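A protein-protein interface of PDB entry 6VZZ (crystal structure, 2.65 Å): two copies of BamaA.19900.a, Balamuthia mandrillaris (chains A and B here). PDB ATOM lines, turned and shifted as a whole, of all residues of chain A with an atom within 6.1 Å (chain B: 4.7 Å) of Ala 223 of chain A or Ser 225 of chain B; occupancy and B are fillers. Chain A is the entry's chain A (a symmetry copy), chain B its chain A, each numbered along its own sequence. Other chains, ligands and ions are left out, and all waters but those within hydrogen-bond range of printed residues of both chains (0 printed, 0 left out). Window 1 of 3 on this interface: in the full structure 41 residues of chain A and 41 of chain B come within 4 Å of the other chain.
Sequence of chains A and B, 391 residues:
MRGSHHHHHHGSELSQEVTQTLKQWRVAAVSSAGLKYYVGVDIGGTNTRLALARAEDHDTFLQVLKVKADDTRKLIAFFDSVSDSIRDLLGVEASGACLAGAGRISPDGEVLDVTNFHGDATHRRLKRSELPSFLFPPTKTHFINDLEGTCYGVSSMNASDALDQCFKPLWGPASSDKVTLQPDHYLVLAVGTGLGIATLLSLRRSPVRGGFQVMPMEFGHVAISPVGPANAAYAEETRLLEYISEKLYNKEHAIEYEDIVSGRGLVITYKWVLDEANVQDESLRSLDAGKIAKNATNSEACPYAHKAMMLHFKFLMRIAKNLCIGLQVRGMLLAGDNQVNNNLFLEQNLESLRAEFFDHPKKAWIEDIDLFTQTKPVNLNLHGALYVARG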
ATOM      1  N   HIS A 221      22.318  11.085   9.537  1.00  0.00           N
ATOM      2  CA  HIS A 221      23.619  10.778   8.973  1.00  0.00           C
ATOM      3  C   HIS A 221      23.588  10.554   7.465  1.00  0.00           C
ATOM      4  O   HIS A 221      24.621  10.210   6.887  1.00  0.00           O
ATOM      5  CB  HIS A 221      24.211   9.569   9.699  1.00  0.00           C
ATOM      6  CG  HIS A 221      24.303   9.763  11.180  1.00  0.00           C
ATOM      7  ND1 HIS A 221      25.241  10.589  11.765  1.00  0.00           N
ATOM      8  CD2 HIS A 221      23.558   9.262  12.195  1.00  0.00           C
ATOM      9  CE1 HIS A 221      25.076  10.580  13.076  1.00  0.00           C
ATOM     10  NE2 HIS A 221      24.064   9.782  13.362  1.00  0.00           N
ATOM     11  N   VAL A 222      22.443  10.760   6.802  1.00  0.00           N
ATOM     12  CA  VAL A 222      22.409  10.635   5.347  1.00  0.00           C
ATOM     13  C   VAL A 222      23.046  11.865   4.709  1.00  0.00           C
ATOM     14  O   VAL A 222      23.044  12.968   5.273  1.00  0.00           O
ATOM     15  CB  VAL A 222      20.971  10.423   4.828  1.00  0.00           C
ATOM     16  CG1 VAL A 222      20.328   9.213   5.483  1.00  0.00           C
ATOM     17  CG2 VAL A 222      20.133  11.684   4.998  1.00  0.00           C
ATOM     18  N   ALA A 223      23.605  11.667   3.517  1.00  0.00           N
ATOM     19  CA  ALA A 223      24.209  12.762   2.774  1.00  0.00           C
ATOM     20  C   ALA A 223      23.184  13.845   2.464  1.00  0.00           C
ATOM     21  O   ALA A 223      22.001  13.566   2.244  1.00  0.00           O
ATOM     22  CB  ALA A 223      24.813  12.238   1.478  1.00  0.00           C
ATOM     23  N   ILE A 224      23.647  15.091   2.436  1.00  0.00           N
ATOM     24  CA  ILE A 224      22.780  16.235   2.188  1.00  0.00           C
ATOM     25  C   ILE A 224      22.330  16.268   0.731  1.00  0.00           C
ATOM     26  O   ILE A 224      22.880  15.565  -0.123  1.00  0.00           O
ATOM     27  CB  ILE A 224      23.502  17.540   2.568  1.00  0.00           C
ATOM     28  CG1 ILE A 224      24.895  17.581   1.944  1.00  0.00           C
ATOM     29  CG2 ILE A 224      23.638  17.639   4.069  1.00  0.00           C
ATOM     30  CD1 ILE A 224      24.930  18.066   0.538  1.00  0.00           C
ATOM     31  N   SER A 225      21.349  17.115   0.440  1.00  0.00           N
ATOM     32  CA  SER A 225      20.925  17.433  -0.907  1.00  0.00           C
ATOM     33  C   SER A 225      21.255  18.881  -1.246  1.00  0.00           C
ATOM     34  O   SER A 225      21.231  19.746  -0.368  1.00  0.00           O
ATOM     35  CB  SER A 225      19.419  17.204  -1.059  1.00  0.00           C
ATOM     36  OG  SER A 225      19.166  15.836  -1.283  1.00  0.00           O
ATOM     37  N   PRO A 226      21.565  19.184  -2.500  1.00  0.00           N
ATOM     38  CA  PRO A 226      21.845  20.568  -2.895  1.00  0.00           C
ATOM     39  C   PRO A 226      20.540  21.300  -3.189  1.00  0.00           C
ATOM     40  O   PRO A 226      19.460  20.727  -3.105  1.00  0.00           O
ATOM     41  CB  PRO A 226      22.686  20.394  -4.157  1.00  0.00           C
ATOM     42  CG  PRO A 226      22.119  19.185  -4.789  1.00  0.00           C
ATOM     43  CD  PRO A 226      21.695  18.263  -3.643  1.00  0.00           C
ATOM     44  N   ALA A 254      30.600  13.484   0.802  1.00  0.00           N
ATOM     45  CA  ALA A 254      29.547  14.474   0.975  1.00  0.00           C
ATOM     46  C   ALA A 254      29.098  14.485   2.428  1.00  0.00           C
ATOM     47  O   ALA A 254      28.923  13.428   3.041  1.00  0.00           O
ATOM     48  CB  ALA A 254      28.366  14.158   0.061  1.00  0.00           C
ATOM     49  N   ILE A 255      28.901  15.683   2.985  1.00  0.00           N
ATOM     50  CA  ILE A 255      28.655  15.777   4.426  1.00  0.00           C
ATOM     51  C   ILE A 255      27.271  15.234   4.775  1.00  0.00           C
ATOM     52  O   ILE A 255      26.367  15.131   3.935  1.00  0.00           O
ATOM     53  CB  ILE A 255      28.833  17.220   4.926  1.00  0.00           C
ATOM     54  CG1 ILE A 255      27.662  18.108   4.520  1.00  0.00           C
ATOM     55  CG2 ILE A 255      30.112  17.813   4.375  1.00  0.00           C
ATOM     56  CD1 ILE A 255      27.746  19.506   5.143  1.00  0.00           C
ATOM     57  N   GLU A 256      27.119  14.847   6.036  1.00  0.00           N
ATOM     58  CA  GLU A 256      25.835  14.418   6.572  1.00  0.00           C
ATOM     59  C   GLU A 256      25.040  15.634   7.001  1.00  0.00           C
ATOM     60  O   GLU A 256      25.603  16.688   7.312  1.00  0.00           O
ATOM     61  CB  GLU A 256      26.008  13.490   7.782  1.00  0.00           C
ATOM     62  CG  GLU A 256      27.060  12.415   7.636  1.00  0.00           C
ATOM     63  CD  GLU A 256      27.181  11.558   8.882  1.00  0.00           C
ATOM     64  OE1 GLU A 256      26.735  12.004   9.966  1.00  0.00           O
ATOM     65  OE2 GLU A 256      27.712  10.429   8.778  1.00  0.00           O
ATOM     66  N   TYR A 257      23.711  15.480   7.022  1.00  0.00           N
ATOM     67  CA  TYR A 257      22.868  16.567   7.511  1.00  0.00           C
ATOM     68  C   TYR A 257      23.290  16.986   8.915  1.00  0.00           C
ATOM     69  O   TYR A 257      23.290  18.182   9.238  1.00  0.00           O
ATOM     70  CB  TYR A 257      21.393  16.166   7.483  1.00  0.00           C
ATOM     71  CG  TYR A 257      20.717  16.387   6.143  1.00  0.00           C
ATOM     72  CD1 TYR A 257      20.356  17.663   5.726  1.00  0.00           C
ATOM     73  CD2 TYR A 257      20.434  15.319   5.295  1.00  0.00           C
ATOM     74  CE1 TYR A 257      19.736  17.867   4.503  1.00  0.00           C
ATOM     75  CE2 TYR A 257      19.819  15.519   4.079  1.00  0.00           C
ATOM     76  CZ  TYR A 257      19.474  16.795   3.682  1.00  0.00           C
ATOM     77  OH  TYR A 257      18.855  16.998   2.463  1.00  0.00           O
ATOM     78  N   ALA B 223      15.207  14.500  -3.232  1.00  0.00           N
ATOM     79  CA  ALA B 223      16.329  15.126  -3.915  1.00  0.00           C
ATOM     80  C   ALA B 223      17.586  14.274  -3.796  1.00  0.00           C
ATOM     81  O   ALA B 223      17.812  13.599  -2.786  1.00  0.00           O
ATOM     82  CB  ALA B 223      16.586  16.508  -3.331  1.00  0.00           C
ATOM     83  N   ILE B 224      18.414  14.315  -4.835  1.00  0.00           N
ATOM     84  CA  ILE B 224      19.638  13.527  -4.882  1.00  0.00           C
ATOM     85  C   ILE B 224      20.676  14.079  -3.911  1.00  0.00           C
ATOM     86  O   ILE B 224      20.541  15.196  -3.399  1.00  0.00           O
ATOM     87  CB  ILE B 224      20.193  13.494  -6.317  1.00  0.00           C
ATOM     88  CG1 ILE B 224      20.258  14.905  -6.897  1.00  0.00           C
ATOM     89  CG2 ILE B 224      19.306  12.647  -7.197  1.00  0.00           C
ATOM     90  CD1 ILE B 224      21.479  15.672  -6.528  1.00  0.00           C
ATOM     91  N   SER B 225      21.735  13.310  -3.684  1.00  0.00           N
ATOM     92  CA  SER B 225      22.910  13.741  -2.958  1.00  0.00           C
ATOM     93  C   SER B 225      24.115  13.822  -3.887  1.00  0.00           C
ATOM     94  O   SER B 225      24.223  13.041  -4.834  1.00  0.00           O
ATOM     95  CB  SER B 225      23.214  12.771  -1.812  1.00  0.00           C
ATOM     96  OG  SER B 225      22.397  13.073  -0.704  1.00  0.00           O
ATOM     97  N   PRO B 226      25.037  14.746  -3.650  1.00  0.00           N
ATOM     98  CA  PRO B 226      26.241  14.842  -4.481  1.00  0.00           C
ATOM     99  C   PRO B 226      27.298  13.862  -3.981  1.00  0.00           C
ATOM    100  O   PRO B 226      27.092  13.153  -3.004  1.00  0.00           O
ATOM    101  CB  PRO B 226      26.679  16.289  -4.275  1.00  0.00           C
ATOM    102  CG  PRO B 226      26.311  16.568  -2.871  1.00  0.00           C
ATOM    103  CD  PRO B 226      25.024  15.783  -2.604  1.00  0.00           C
ATOM    104  N   VAL B 227      28.438  13.821  -4.677  1.00  0.00           N
ATOM    105  CA  VAL B 227      29.606  13.116  -4.156  1.00  0.00           C
ATOM    106  C   VAL B 227      30.465  14.103  -3.387  1.00  0.00           C
ATOM    107  O   VAL B 227      30.193  15.312  -3.382  1.00  0.00           O
ATOM    108  CB  VAL B 227      30.451  12.458  -5.263  1.00  0.00           C
ATOM    109  CG1 VAL B 227      29.745  11.282  -5.859  1.00  0.00           C
ATOM    110  CG2 VAL B 227      30.819  13.482  -6.333  1.00  0.00           C
ATOM    111  N   TYR B 257      15.856  11.440  -7.361  1.00  0.00           N
ATOM    112  CA  TYR B 257      16.576  10.231  -7.749  1.00  0.00           C
ATOM    113  C   TYR B 257      15.915   9.574  -8.955  1.00  0.00           C
ATOM    114  O   TYR B 257      16.607   9.067  -9.849  1.00  0.00           O
ATOM    115  CB  TYR B 257      16.667   9.253  -6.578  1.00  0.00           C
ATOM    116  CG  TYR B 257      17.830   9.517  -5.640  1.00  0.00           C
ATOM    117  CD1 TYR B 257      19.129   9.176  -5.998  1.00  0.00           C
ATOM    118  CD2 TYR B 257      17.630  10.103  -4.393  1.00  0.00           C
ATOM    119  CE1 TYR B 257      20.193   9.414  -5.140  1.00  0.00           C
ATOM    120  CE2 TYR B 257      18.684  10.342  -3.540  1.00  0.00           C
ATOM    121  CZ  TYR B 257      19.967  10.000  -3.918  1.00  0.00           C
ATOM    122  OH  TYR B 257      21.028  10.237  -3.062  1.00  0.00           O
ATOM    123  N   PHE B 315      23.521   6.111  -9.100  1.00  0.00           N
ATOM    124  CA  PHE B 315      22.559   6.832  -8.278  1.00  0.00           C
ATOM    125  C   PHE B 315      21.577   5.890  -7.606  1.00  0.00           C
ATOM    126  O   PHE B 315      21.072   6.205  -6.524  1.00  0.00           O
ATOM    127  CB  PHE B 315      21.831   7.889  -9.102  1.00  0.00           C
ATOM    128  CG  PHE B 315      22.594   9.169  -9.219  1.00  0.00           C
ATOM    129  CD1 PHE B 315      23.596   9.309 -10.172  1.00  0.00           C
ATOM    130  CD2 PHE B 315      22.339  10.223  -8.355  1.00  0.00           C
ATOM    131  CE1 PHE B 315      24.323  10.488 -10.271  1.00  0.00           C
ATOM    132  CE2 PHE B 315      23.054  11.397  -8.445  1.00  0.00           C
ATOM    133  CZ  PHE B 315      24.050  11.536  -9.407  1.00  0.00           C
ATOM    134  N   ARG B 318      23.396   5.099  -4.596  1.00  0.00           N
ATOM    135  CA  ARG B 318      23.496   6.197  -3.634  1.00  0.00           C
ATOM    136  C   ARG B 318      22.230   6.328  -2.792  1.00  0.00           C
ATOM    137  O   ARG B 318      22.311   6.559  -1.579  1.00  0.00           O
ATOM    138  CB  ARG B 318      23.790   7.512  -4.343  1.00  0.00           C
ATOM    139  CG  ARG B 318      24.006   8.661  -3.381  1.00  0.00           C
ATOM    140  CD  ARG B 318      24.695   9.826  -4.072  1.00  0.00           C
ATOM    141  NE  ARG B 318      25.788   9.346  -4.905  1.00  0.00           N
ATOM    142  CZ  ARG B 318      26.384  10.057  -5.856  1.00  0.00           C
ATOM    143  NH1 ARG B 318      27.353   9.508  -6.574  1.00  0.00           N
ATOM    144  NH2 ARG B 318      25.999  11.304  -6.102  1.00  0.00           N
ATOM    145  N   ASN B 322      22.000   5.529   1.425  1.00  0.00           N
ATOM    146  CA  ASN B 322      21.479   6.435   2.443  1.00  0.00           C
ATOM    147  C   ASN B 322      20.219   5.898   3.121  1.00  0.00           C
ATOM    148  O   ASN B 322      20.007   6.155   4.315  1.00  0.00           O
ATOM    149  CB  ASN B 322      21.251   7.804   1.823  1.00  0.00           C
ATOM    150  CG  ASN B 322      22.562   8.544   1.632  1.00  0.00           C
ATOM    151  OD1 ASN B 322      23.132   9.068   2.594  1.00  0.00           O
ATOM    152  ND2 ASN B 322      23.082   8.543   0.406  1.00  0.00           N
ATOM    153  N   HIS B 360      30.698   6.609   2.228  1.00  0.00           N
ATOM    154  CA  HIS B 360      29.954   7.275   3.293  1.00  0.00           C
ATOM    155  C   HIS B 360      30.828   7.353   4.533  1.00  0.00           C
ATOM    156  O   HIS B 360      31.616   6.436   4.790  1.00  0.00           O
ATOM    157  CB  HIS B 360      28.645   6.532   3.611  1.00  0.00           C
ATOM    158  CG  HIS B 360      27.618   7.392   4.283  1.00  0.00           C
ATOM    159  ND1 HIS B 360      27.634   7.645   5.639  1.00  0.00           N
ATOM    160  CD2 HIS B 360      26.556   8.071   3.785  1.00  0.00           C
ATOM    161  CE1 HIS B 360      26.631   8.446   5.946  1.00  0.00           C
ATOM    162  NE2 HIS B 360      25.955   8.713   4.842  1.00  0.00           N
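Among the printed residues, merely in contact across the chains: Val 222 of chain A with Asn 322 of chain B, Pro 226 of chain A with Ile 224 of chain B, Ile 224 of chain A with Pro 226 of chain B, Ala 254 of chain A with Pro 226 of chain B and Glu 256 of chain A with His 360 of chain B.
Printed residues of chain B within 4 Å of Val 222 of chain A: Asn 322 (3.2 Å). Of the printed residues of chain A, Pro 226 of chain B touches Ile 224 (3.3 Å) and Ala 254 (3.5 Å). Of the printed residues of chain A, Asn 322 of chain B touches Val 222 and Ala 223.
Ala 223 of chain A touches Ser 225 of chain B, and with the chains exchanged Ser 225 of chain A touches Ala 223 of chain B. Ile 224 of chain A touches Ser 225 of chain B, and with the chains exchanged Ser 225 of chain A touches Ile 224 of chain B. Ile 224 of chain A touches Pro 226 of chain B, and with the chains exchanged Pro 226 of chain A touches Ile 224 of chain B. Of the 11 pairs that touch across the chains among the printed residues, 6 have their exchanged pair printed and touching as well.
The side-chain hydroxyl (OG) of Ser 225 of chain B lies within hydrogen-bond range of the backbone carbonyl oxygen (O) of Ala 223 of chain A. The backbone carbonyl oxygen (O) of His 221 of chain A sits close to a ring nitrogen (NE2) of His 360 of chain B, 2.9 Å away. OG of Ser 225 of chain B lies within hydrogen-bond range of O of Ile 224 of chain A, at 2.6 Å. The backbone carbonyl oxygen of Ile 224 of chain B lies within hydrogen-bond range of the side-chain hydroxyl of Ser 225 of chain A (2.6 Å). The side-chain hydroxyl (OG) of Ser 225 of chain A lies within hydrogen-bond range of the backbone carbonyl oxygen (O) of Ala 223 of chain B (3.0 Å). The side-chain amide oxygen of Asn 322 of chain B sits at hydrogen-bond distance from the backbone NH of Ala 223 of chain A, at 2.8 Å.
The backbone carbonyl oxygen of Arg 318 of chain B is in hydrogen-bond range of the side-chain amide nitrogen of Asn 322 of chain B. The backbone NH (N) of Ser 225 of chain A sits at hydrogen-bond distance from the side-chain hydroxyl (OH) of Tyr 257 of chain A, at 3.2 Å. N of Ser 225 of chain B lies within hydrogen-bond range of OH of Tyr 257 of chain B (3.2 Å). The backbone NH (N) of Ile 224 of chain A lies within hydrogen-bond range of the backbone carbonyl oxygen (O) of Ile 255 of chain A, 3.1 Å away. OE1 of Glu 256 of chain A sits at hydrogen-bond distance from ND1 of His 221 of chain A (2.7 Å). O of Val 222 of chain A sits at hydrogen-bond distance from N of Tyr 257 of chain A (3.1 Å).
Hydrophobic or aromatic side chains of chain B that line the printed part of chain A: Ala 223, Ile 224, Pro 226 and His 360.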
